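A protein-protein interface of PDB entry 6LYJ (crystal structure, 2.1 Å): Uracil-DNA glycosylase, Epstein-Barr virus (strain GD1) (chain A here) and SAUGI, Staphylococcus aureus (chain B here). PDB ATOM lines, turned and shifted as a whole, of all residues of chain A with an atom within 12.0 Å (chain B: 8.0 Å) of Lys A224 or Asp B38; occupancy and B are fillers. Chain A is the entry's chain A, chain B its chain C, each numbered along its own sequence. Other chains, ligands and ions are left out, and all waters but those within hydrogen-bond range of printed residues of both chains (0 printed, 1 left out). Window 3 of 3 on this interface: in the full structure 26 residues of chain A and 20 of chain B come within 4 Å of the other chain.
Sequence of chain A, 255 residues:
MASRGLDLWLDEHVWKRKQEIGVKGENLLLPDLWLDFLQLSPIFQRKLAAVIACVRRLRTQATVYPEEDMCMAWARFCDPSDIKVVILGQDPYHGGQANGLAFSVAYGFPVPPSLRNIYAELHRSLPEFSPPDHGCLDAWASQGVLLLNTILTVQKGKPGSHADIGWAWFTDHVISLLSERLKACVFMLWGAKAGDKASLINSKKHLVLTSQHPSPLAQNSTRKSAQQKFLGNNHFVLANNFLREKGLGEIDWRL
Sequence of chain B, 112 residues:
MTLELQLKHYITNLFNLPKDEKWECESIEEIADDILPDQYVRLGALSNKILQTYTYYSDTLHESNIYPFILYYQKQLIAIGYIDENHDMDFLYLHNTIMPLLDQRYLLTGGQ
OD1 of Asp B38 is in salt-bridge range of NZ of Lys A224, 3.95 Å away.
OG of Ser A221 lies within hydrogen-bond range of O of Asp B34 (2.9 Å).
The side-chain carboxylate (OD2) of Asp B33 is in salt-bridge range of the side-chain amino group (NZ) of Lys A224 (3.9 Å).
O of Leu A217 lies close to O of Ile B35.
NE2 of Gln A212 lies close to OD1 of Asp B34 (3.3 Å).
OD2 of Asp B33 sits at hydrogen-bond distance from OG of Ser B47.
O of Ala A218 lies within hydrogen-bond range of NZ of Lys A229 (3.2 Å).
The backbone NH (N) of Gln A212 sits at hydrogen-bond distance from the backbone carbonyl oxygen (O) of Gln A228, at 2.9 Å.
OG of Ser A221 sits close to NZ of Lys A229, 3.2 Å away.
NE2 of Gln A212 lies within hydrogen-bond range of OG of Ser A225.
The backbone carbonyl oxygen (O) of Ala A218 sits close to the side-chain amide oxygen (OE1) of Gln A212, at 3.5 Å.
Among the printed residues, pairs that only touch across the chains: Ala A218 with Asp B34 (3.3 Å), Thr A222 with Asp B38 (3.4 Å), Leu A217 with Asp B34 (3.8 Å), Ala A218 with Ile B35 (3.8 Å) and Ser A225 with Asp B34 (3.9 Å).
Of chain B, only Asp B33 (3.9 Å) and Asp B38 (3.9 Å) come within 4 Å of Lys A224.
Of chain A, only Thr A222 and Lys A224 come within 4 Å of Asp B38.
Asp B33 touches just one residue of chain A: Lys A224 (3.9 Å).
No residue of chain A comes within 4 Å of Pro B37.
No residue of chain A comes within 4 Å of Val B41.
Of the printed residues of chain A, Asp B34 touches Gln A212, Leu A217, Ala A218, Ser A221 and Ser A225.
Of the printed residues of chain B, Gln A212 touches Asp B34.
Of the printed residues of chain A, Ile B35 touches Leu A217 (3.3 Å) and Ala A218 (3.8 Å).
Of the printed residues of chain B, Ser A221 touches Asp B34.
Asn B48 touches none of the printed residues of chain A.
Of the 14 printed residues of chain B, 4 touch a printed residue of chain A.
Printed residues of chain B that touch a printed residue of chain A: Asp B33, Asp B34, Ile B35 and Asp B38.
Hydrophobic or aromatic side chains of chain B within 4 Å of the printed part of chain A: Ile B35.
Among the printed residues, Asp or Glu carboxylates within 4 Å of a Lys or Arg side-chain nitrogen of the other chain: Lys A224 with Asp B33 and Lys A224 with Asp B38.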
ATOM      1  N   SER A 211      21.193   8.218 -16.034  1.00  0.00           N
ATOM      2  CA  SER A 211      20.716   8.409 -17.399  1.00  0.00           C
ATOM      3  C   SER A 211      20.725   9.902 -17.688  1.00  0.00           C
ATOM      4  O   SER A 211      21.031  10.725 -16.817  1.00  0.00           O
ATOM      5  CB  SER A 211      19.320   7.815 -17.604  1.00  0.00           C
ATOM      6  OG  SER A 211      18.321   8.651 -17.045  1.00  0.00           O
ATOM      7  N   GLN A 212      20.373  10.248 -18.923  1.00  0.00           N
ATOM      8  CA  GLN A 212      20.132  11.642 -19.254  1.00  0.00           C
ATOM      9  C   GLN A 212      18.929  12.171 -18.482  1.00  0.00           C
ATOM     10  O   GLN A 212      18.114  11.417 -17.946  1.00  0.00           O
ATOM     11  CB  GLN A 212      19.908  11.810 -20.754  1.00  0.00           C
ATOM     12  CG  GLN A 212      21.182  11.736 -21.565  1.00  0.00           C
ATOM     13  CD  GLN A 212      20.948  12.047 -23.023  1.00  0.00           C
ATOM     14  OE1 GLN A 212      19.869  11.797 -23.556  1.00  0.00           O
ATOM     15  NE2 GLN A 212      21.958  12.605 -23.678  1.00  0.00           N
ATOM     16  N   LEU A 217      13.959  18.959 -23.223  1.00  0.00           N
ATOM     17  CA  LEU A 217      15.112  19.503 -23.937  1.00  0.00           C
ATOM     18  C   LEU A 217      16.150  18.430 -24.239  1.00  0.00           C
ATOM     19  O   LEU A 217      16.835  18.501 -25.266  1.00  0.00           O
ATOM     20  CB  LEU A 217      15.743  20.631 -23.119  1.00  0.00           C
ATOM     21  CG  LEU A 217      14.864  21.839 -22.792  1.00  0.00           C
ATOM     22  CD1 LEU A 217      15.619  22.817 -21.918  1.00  0.00           C
ATOM     23  CD2 LEU A 217      14.394  22.526 -24.065  1.00  0.00           C
ATOM     24  N   ALA A 218      16.302  17.450 -23.349  1.00  0.00           N
ATOM     25  CA  ALA A 218      17.263  16.371 -23.526  1.00  0.00           C
ATOM     26  C   ALA A 218      16.645  15.119 -24.136  1.00  0.00           C
ATOM     27  O   ALA A 218      17.327  14.094 -24.236  1.00  0.00           O
ATOM     28  CB  ALA A 218      17.915  16.025 -22.185  1.00  0.00           C
ATOM     29  N   GLN A 219      15.373  15.172 -24.535  1.00  0.00           N
ATOM     30  CA  GLN A 219      14.660  13.958 -24.924  1.00  0.00           C
ATOM     31  C   GLN A 219      15.139  13.446 -26.276  1.00  0.00           C
ATOM     32  O   GLN A 219      15.683  12.341 -26.381  1.00  0.00           O
ATOM     33  CB  GLN A 219      13.153  14.211 -24.948  1.00  0.00           C
ATOM     34  CG  GLN A 219      12.348  13.045 -25.502  1.00  0.00           C
ATOM     35  CD  GLN A 219      10.952  12.962 -24.920  1.00  0.00           C
ATOM     36  OE1 GLN A 219      10.777  12.842 -23.706  1.00  0.00           O
ATOM     37  NE2 GLN A 219       9.946  13.023 -25.786  1.00  0.00           N
ATOM     38  N   ASN A 220      14.931  14.231 -27.331  1.00  0.00           N
ATOM     39  CA  ASN A 220      15.389  13.877 -28.668  1.00  0.00           C
ATOM     40  C   ASN A 220      16.701  14.597 -28.937  1.00  0.00           C
ATOM     41  O   ASN A 220      16.759  15.829 -28.878  1.00  0.00           O
ATOM     42  CB  ASN A 220      14.345  14.256 -29.717  1.00  0.00           C
ATOM     43  CG  ASN A 220      14.195  13.206 -30.798  1.00  0.00           C
ATOM     44  OD1 ASN A 220      14.266  13.511 -31.989  1.00  0.00           O
ATOM     45  ND2 ASN A 220      13.983  11.960 -30.388  1.00  0.00           N
ATOM     46  N   SER A 221      17.747  13.830 -29.238  1.00  0.00           N
ATOM     47  CA  SER A 221      19.076  14.413 -29.369  1.00  0.00           C
ATOM     48  C   SER A 221      19.921  13.694 -30.411  1.00  0.00           C
ATOM     49  O   SER A 221      19.588  13.674 -31.601  1.00  0.00           O
ATOM     50  CB  SER A 221      19.803  14.416 -28.024  1.00  0.00           C
ATOM     51  OG  SER A 221      19.148  15.252 -27.086  1.00  0.00           O
ATOM     52  N   THR A 222      21.018  13.099 -29.955  1.00  0.00           N
ATOM     53  CA  THR A 222      22.054  12.544 -30.811  1.00  0.00           C
ATOM     54  C   THR A 222      22.258  11.063 -30.522  1.00  0.00           C
ATOM     55  O   THR A 222      22.308  10.651 -29.359  1.00  0.00           O
ATOM     56  CB  THR A 222      23.377  13.282 -30.597  1.00  0.00           C
ATOM     57  OG1 THR A 222      23.791  13.131 -29.233  1.00  0.00           O
ATOM     58  CG2 THR A 222      23.193  14.756 -30.868  1.00  0.00           C
ATOM     59  N   ARG A 223      22.371  10.265 -31.585  1.00  0.00           N
ATOM     60  CA  ARG A 223      22.865   8.901 -31.435  1.00  0.00           C
ATOM     61  C   ARG A 223      24.366   8.972 -31.172  1.00  0.00           C
ATOM     62  O   ARG A 223      25.177   8.474 -31.961  1.00  0.00           O
ATOM     63  CB  ARG A 223      22.565   8.053 -32.674  1.00  0.00           C
ATOM     64  CG  ARG A 223      21.182   7.411 -32.694  1.00  0.00           C
ATOM     65  CD  ARG A 223      20.074   8.423 -32.931  1.00  0.00           C
ATOM     66  NE  ARG A 223      18.766   7.883 -32.570  1.00  0.00           N
ATOM     67  CZ  ARG A 223      17.959   7.252 -33.417  1.00  0.00           C
ATOM     68  NH1 ARG A 223      18.326   7.077 -34.680  1.00  0.00           N
ATOM     69  NH2 ARG A 223      16.786   6.792 -33.002  1.00  0.00           N
ATOM     70  N   LYS A 224      24.726   9.600 -30.053  1.00  0.00           N
ATOM     71  CA  LYS A 224      26.097   9.928 -29.686  1.00  0.00           C
ATOM     72  C   LYS A 224      26.286   9.838 -28.180  1.00  0.00           C
ATOM     73  O   LYS A 224      27.303   9.324 -27.701  1.00  0.00           O
ATOM     74  CB  LYS A 224      26.438  11.343 -30.156  1.00  0.00           C
ATOM     75  CG  LYS A 224      27.616  11.971 -29.427  1.00  0.00           C
ATOM     76  CD  LYS A 224      27.701  13.463 -29.701  1.00  0.00           C
ATOM     77  CE  LYS A 224      28.907  14.084 -29.013  1.00  0.00           C
ATOM     78  NZ  LYS A 224      29.044  15.534 -29.326  1.00  0.00           N
ATOM     79  N   SER A 225      25.304  10.358 -27.440  1.00  0.00           N
ATOM     80  CA  SER A 225      25.296  10.395 -25.982  1.00  0.00           C
ATOM     81  C   SER A 225      25.816   9.116 -25.340  1.00  0.00           C
ATOM     82  O   SER A 225      25.163   8.069 -25.403  1.00  0.00           O
ATOM     83  CB  SER A 225      23.879  10.680 -25.476  1.00  0.00           C
ATOM     84  OG  SER A 225      23.473  11.997 -25.803  1.00  0.00           O
ATOM     85  N   ALA A 226      27.010   9.196 -24.743  1.00  0.00           N
ATOM     86  CA  ALA A 226      27.536   8.083 -23.963  1.00  0.00           C
ATOM     87  C   ALA A 226      26.534   7.621 -22.915  1.00  0.00           C
ATOM     88  O   ALA A 226      26.498   6.434 -22.567  1.00  0.00           O
ATOM     89  CB  ALA A 226      28.857   8.481 -23.302  1.00  0.00           C
ATOM     90  N   GLN A 227      25.719   8.539 -22.402  1.00  0.00           N
ATOM     91  CA  GLN A 227      24.689   8.207 -21.433  1.00  0.00           C
ATOM     92  C   GLN A 227      23.407   7.757 -22.119  1.00  0.00           C
ATOM     93  O   GLN A 227      23.029   8.256 -23.182  1.00  0.00           O
ATOM     94  CB  GLN A 227      24.389   9.401 -20.530  1.00  0.00           C
ATOM     95  CG  GLN A 227      25.126   9.375 -19.211  1.00  0.00           C
ATOM     96  CD  GLN A 227      24.362  10.092 -18.124  1.00  0.00           C
ATOM     97  OE1 GLN A 227      23.758  11.137 -18.364  1.00  0.00           O
ATOM     98  NE2 GLN A 227      24.373   9.532 -16.921  1.00  0.00           N
ATOM     99  N   GLN A 228      22.729   6.819 -21.471  1.00  0.00           N
ATOM    100  CA  GLN A 228      21.453   6.306 -21.937  1.00  0.00           C
ATOM    101  C   GLN A 228      20.369   7.379 -21.837  1.00  0.00           C
ATOM    102  O   GLN A 228      20.405   8.250 -20.963  1.00  0.00           O
ATOM    103  CB  GLN A 228      21.095   5.059 -21.129  1.00  0.00           C
ATOM    104  CG  GLN A 228      19.639   4.850 -20.824  1.00  0.00           C
ATOM    105  CD  GLN A 228      19.394   3.522 -20.148  1.00  0.00           C
ATOM    106  OE1 GLN A 228      19.781   3.321 -18.996  1.00  0.00           O
ATOM    107  NE2 GLN A 228      18.755   2.602 -20.862  1.00  0.00           N
ATOM    108  N   LYS A 229      19.421   7.335 -22.772  1.00  0.00           N
ATOM    109  CA  LYS A 229      18.290   8.254 -22.743  1.00  0.00           C
ATOM    110  C   LYS A 229      17.404   7.997 -21.529  1.00  0.00           C
ATOM    111  O   LYS A 229      17.316   6.875 -21.022  1.00  0.00           O
ATOM    112  CB  LYS A 229      17.453   8.098 -24.014  1.00  0.00           C
ATOM    113  CG  LYS A 229      18.094   8.689 -25.242  1.00  0.00           C
ATOM    114  CD  LYS A 229      17.875  10.178 -25.260  1.00  0.00           C
ATOM    115  CE  LYS A 229      18.457  10.814 -26.499  1.00  0.00           C
ATOM    116  NZ  LYS A 229      18.978  12.159 -26.152  1.00  0.00           N
ATOM    117  N   PHE A 230      16.741   9.055 -21.053  1.00  0.00           N
ATOM    118  CA  PHE A 230      15.826   8.884 -19.930  1.00  0.00           C
ATOM    119  C   PHE A 230      14.706   7.916 -20.292  1.00  0.00           C
ATOM    120  O   PHE A 230      14.490   6.912 -19.605  1.00  0.00           O
ATOM    121  CB  PHE A 230      15.251  10.223 -19.472  1.00  0.00           C
ATOM    122  CG  PHE A 230      14.382  10.100 -18.251  1.00  0.00           C
ATOM    123  CD1 PHE A 230      14.938  10.158 -16.984  1.00  0.00           C
ATOM    124  CD2 PHE A 230      13.018   9.875 -18.371  1.00  0.00           C
ATOM    125  CE1 PHE A 230      14.145  10.021 -15.856  1.00  0.00           C
ATOM    126  CE2 PHE A 230      12.221   9.739 -17.251  1.00  0.00           C
ATOM    127  CZ  PHE A 230      12.784   9.810 -15.991  1.00  0.00           C
ATOM    128  N   ALA B  32      25.305  21.532 -22.986  1.00  0.00           N
ATOM    129  CA  ALA B  32      24.697  21.828 -24.281  1.00  0.00           C
ATOM    130  C   ALA B  32      24.634  20.598 -25.175  1.00  0.00           C
ATOM    131  O   ALA B  32      23.714  20.472 -25.993  1.00  0.00           O
ATOM    132  CB  ALA B  32      25.470  22.948 -24.978  1.00  0.00           C
ATOM    133  N   ASP B  33      25.593  19.678 -25.023  1.00  0.00           N
ATOM    134  CA  ASP B  33      25.651  18.499 -25.883  1.00  0.00           C
ATOM    135  C   ASP B  33      24.401  17.635 -25.770  1.00  0.00           C
ATOM    136  O   ASP B  33      24.045  16.937 -26.728  1.00  0.00           O
ATOM    137  CB  ASP B  33      26.890  17.667 -25.545  1.00  0.00           C
ATOM    138  CG  ASP B  33      28.170  18.471 -25.620  1.00  0.00           C
ATOM    139  OD1 ASP B  33      28.318  19.417 -24.816  1.00  0.00           O
ATOM    140  OD2 ASP B  33      29.023  18.162 -26.482  1.00  0.00           O
ATOM    141  N   ASP B  34      23.726  17.656 -24.618  1.00  0.00           N
ATOM    142  CA  ASP B  34      22.550  16.819 -24.416  1.00  0.00           C
ATOM    143  C   ASP B  34      21.240  17.482 -24.820  1.00  0.00           C
ATOM    144  O   ASP B  34      20.217  16.791 -24.891  1.00  0.00           O
ATOM    145  CB  ASP B  34      22.437  16.400 -22.947  1.00  0.00           C
ATOM    146  CG  ASP B  34      23.424  15.321 -22.566  1.00  0.00           C
ATOM    147  OD1 ASP B  34      24.273  14.958 -23.406  1.00  0.00           O
ATOM    148  OD2 ASP B  34      23.333  14.825 -21.422  1.00  0.00           O
ATOM    149  N   ILE B  35      21.228  18.786 -25.079  1.00  0.00           N
ATOM    150  CA  ILE B  35      19.978  19.506 -25.299  1.00  0.00           C
ATOM    151  C   ILE B  35      19.921  20.219 -26.641  1.00  0.00           C
ATOM    152  O   ILE B  35      18.841  20.692 -27.022  1.00  0.00           O
ATOM    153  CB  ILE B  35      19.677  20.498 -24.155  1.00  0.00           C
ATOM    154  CG1 ILE B  35      20.849  21.434 -23.904  1.00  0.00           C
ATOM    155  CG2 ILE B  35      19.340  19.750 -22.865  1.00  0.00           C
ATOM    156  CD1 ILE B  35      20.579  22.402 -22.775  1.00  0.00           C
ATOM    157  N   LEU B  36      21.041  20.355 -27.357  1.00  0.00           N
ATOM    158  CA  LEU B  36      21.004  21.017 -28.648  1.00  0.00           C
ATOM    159  C   LEU B  36      21.309  20.033 -29.776  1.00  0.00           C
ATOM    160  O   LEU B  36      21.966  19.011 -29.553  1.00  0.00           O
ATOM    161  CB  LEU B  36      22.009  22.173 -28.690  1.00  0.00           C
ATOM    162  CG  LEU B  36      21.636  23.348 -27.785  1.00  0.00           C
ATOM    163  CD1 LEU B  36      22.745  24.377 -27.756  1.00  0.00           C
ATOM    164  CD2 LEU B  36      20.345  23.978 -28.263  1.00  0.00           C
ATOM    165  N   PRO B  37      20.819  20.292 -30.991  1.00  0.00           N
ATOM    166  CA  PRO B  37      21.139  19.406 -32.118  1.00  0.00           C
ATOM    167  C   PRO B  37      22.642  19.298 -32.329  1.00  0.00           C
ATOM    168  O   PRO B  37      23.395  20.245 -32.084  1.00  0.00           O
ATOM    169  CB  PRO B  37      20.450  20.076 -33.313  1.00  0.00           C
ATOM    170  CG  PRO B  37      19.386  20.931 -32.716  1.00  0.00           C
ATOM    171  CD  PRO B  37      19.895  21.373 -31.377  1.00  0.00           C
ATOM    172  N   ASP B  38      23.067  18.122 -32.803  1.00  0.00           N
ATOM    173  CA  ASP B  38      24.489  17.806 -32.911  1.00  0.00           C
ATOM    174  C   ASP B  38      25.232  18.828 -33.763  1.00  0.00           C
ATOM    175  O   ASP B  38      26.376  19.189 -33.458  1.00  0.00           O
ATOM    176  CB  ASP B  38      24.658  16.406 -33.501  1.00  0.00           C
ATOM    177  CG  ASP B  38      26.106  15.980 -33.593  1.00  0.00           C
ATOM    178  OD1 ASP B  38      26.780  15.931 -32.542  1.00  0.00           O
ATOM    179  OD2 ASP B  38      26.568  15.693 -34.717  1.00  0.00           O
ATOM    180  N   GLN B  39      24.597  19.308 -34.833  1.00  0.00           N
ATOM    181  CA  GLN B  39      25.260  20.219 -35.757  1.00  0.00           C
ATOM    182  C   GLN B  39      25.603  21.559 -35.119  1.00  0.00           C
ATOM    183  O   GLN B  39      26.449  22.284 -35.651  1.00  0.00           O
ATOM    184  CB  GLN B  39      24.379  20.447 -36.983  1.00  0.00           C
ATOM    185  CG  GLN B  39      23.003  20.991 -36.651  1.00  0.00           C
ATOM    186  CD  GLN B  39      22.147  21.187 -37.882  1.00  0.00           C
ATOM    187  OE1 GLN B  39      22.647  21.564 -38.940  1.00  0.00           O
ATOM    188  NE2 GLN B  39      20.852  20.922 -37.755  1.00  0.00           N
ATOM    189  N   TYR B  40      24.972  21.905 -34.000  1.00  0.00           N
ATOM    190  CA  TYR B  40      25.159  23.204 -33.374  1.00  0.00           C
ATOM    191  C   TYR B  40      26.047  23.141 -32.140  1.00  0.00           C
ATOM    192  O   TYR B  40      26.156  24.134 -31.415  1.00  0.00           O
ATOM    193  CB  TYR B  40      23.799  23.785 -32.988  1.00  0.00           C
ATOM    194  CG  TYR B  40      22.866  24.023 -34.151  1.00  0.00           C
ATOM    195  CD1 TYR B  40      23.315  24.613 -35.328  1.00  0.00           C
ATOM    196  CD2 TYR B  40      21.531  23.651 -34.072  1.00  0.00           C
ATOM    197  CE1 TYR B  40      22.450  24.833 -36.391  1.00  0.00           C
ATOM    198  CE2 TYR B  40      20.664  23.866 -35.124  1.00  0.00           C
ATOM    199  CZ  TYR B  40      21.126  24.455 -36.279  1.00  0.00           C
ATOM    200  OH  TYR B  40      20.248  24.658 -37.316  1.00  0.00           O
ATOM    201  N   VAL B  41      26.691  22.007 -31.892  1.00  0.00           N
ATOM    202  CA  VAL B  41      27.504  21.799 -30.699  1.00  0.00           C
ATOM    203  C   VAL B  41      28.906  21.418 -31.149  1.00  0.00           C
ATOM    204  O   VAL B  41      29.134  20.289 -31.597  1.00  0.00           O
ATOM    205  CB  VAL B  41      26.909  20.727 -29.779  1.00  0.00           C
ATOM    206  CG1 VAL B  41      27.815  20.498 -28.585  1.00  0.00           C
ATOM    207  CG2 VAL B  41      25.521  21.144 -29.321  1.00  0.00           C
ATOM    208  N   ARG B  42      29.849  22.348 -31.026  1.00  0.00           N
ATOM    209  CA  ARG B  42      31.172  22.151 -31.593  1.00  0.00           C
ATOM    210  C   ARG B  42      32.238  22.438 -30.549  1.00  0.00           C
ATOM    211  O   ARG B  42      32.034  23.231 -29.627  1.00  0.00           O
ATOM    212  CB  ARG B  42      31.406  23.062 -32.816  1.00  0.00           C
ATOM    213  CG  ARG B  42      30.492  22.804 -33.999  1.00  0.00           C
ATOM    214  CD  ARG B  42      30.767  21.456 -34.640  1.00  0.00           C
ATOM    215  NE  ARG B  42      29.764  21.111 -35.645  1.00  0.00           N
ATOM    216  CZ  ARG B  42      29.779  21.546 -36.901  1.00  0.00           C
ATOM    217  NH1 ARG B  42      30.741  22.363 -37.313  1.00  0.00           N
ATOM    218  NH2 ARG B  42      28.822  21.179 -37.742  1.00  0.00           N
ATOM    219  N   LEU B  43      33.379  21.773 -30.713  1.00  0.00           N
ATOM    220  CA  LEU B  43      34.530  21.998 -29.850  1.00  0.00           C
ATOM    221  C   LEU B  43      34.975  23.454 -29.932  1.00  0.00           C
ATOM    222  O   LEU B  43      35.021  24.045 -31.015  1.00  0.00           O
ATOM    223  CB  LEU B  43      35.671  21.061 -30.250  1.00  0.00           C
ATOM    224  CG  LEU B  43      35.403  19.576 -29.980  1.00  0.00           C
ATOM    225  CD1 LEU B  43      36.436  18.693 -30.648  1.00  0.00           C
ATOM    226  CD2 LEU B  43      35.375  19.314 -28.482  1.00  0.00           C
ATOM    227  N   SER B  47      30.259  23.096 -27.089  1.00  0.00           N
ATOM    228  CA  SER B  47      30.508  21.765 -26.555  1.00  0.00           C
ATOM    229  C   SER B  47      31.027  21.842 -25.126  1.00  0.00           C
ATOM    230  O   SER B  47      31.925  22.632 -24.819  1.00  0.00           O
ATOM    231  CB  SER B  47      31.500  21.009 -27.432  1.00  0.00           C
ATOM    232  OG  SER B  47      31.717  19.708 -26.921  1.00  0.00           O
ATOM    233  N   ASN B  48      30.429  21.028 -24.252  1.00  0.00           N
ATOM    234  CA  ASN B  48      30.818  20.868 -22.853  1.00  0.00           C
ATOM    235  C   ASN B  48      30.529  22.102 -22.003  1.00  0.00           C
ATOM    236  O   ASN B  48      31.071  22.236 -20.904  1.00  0.00           O
ATOM    237  CB  ASN B  48      32.296  20.474 -22.729  1.00  0.00           C
ATOM    238  CG  ASN B  48      32.592  19.733 -21.444  1.00  0.00           C
ATOM    239  OD1 ASN B  48      33.628  19.947 -20.815  1.00  0.00           O
ATOM    240  ND2 ASN B  48      31.674  18.860 -21.040  1.00  0.00           N
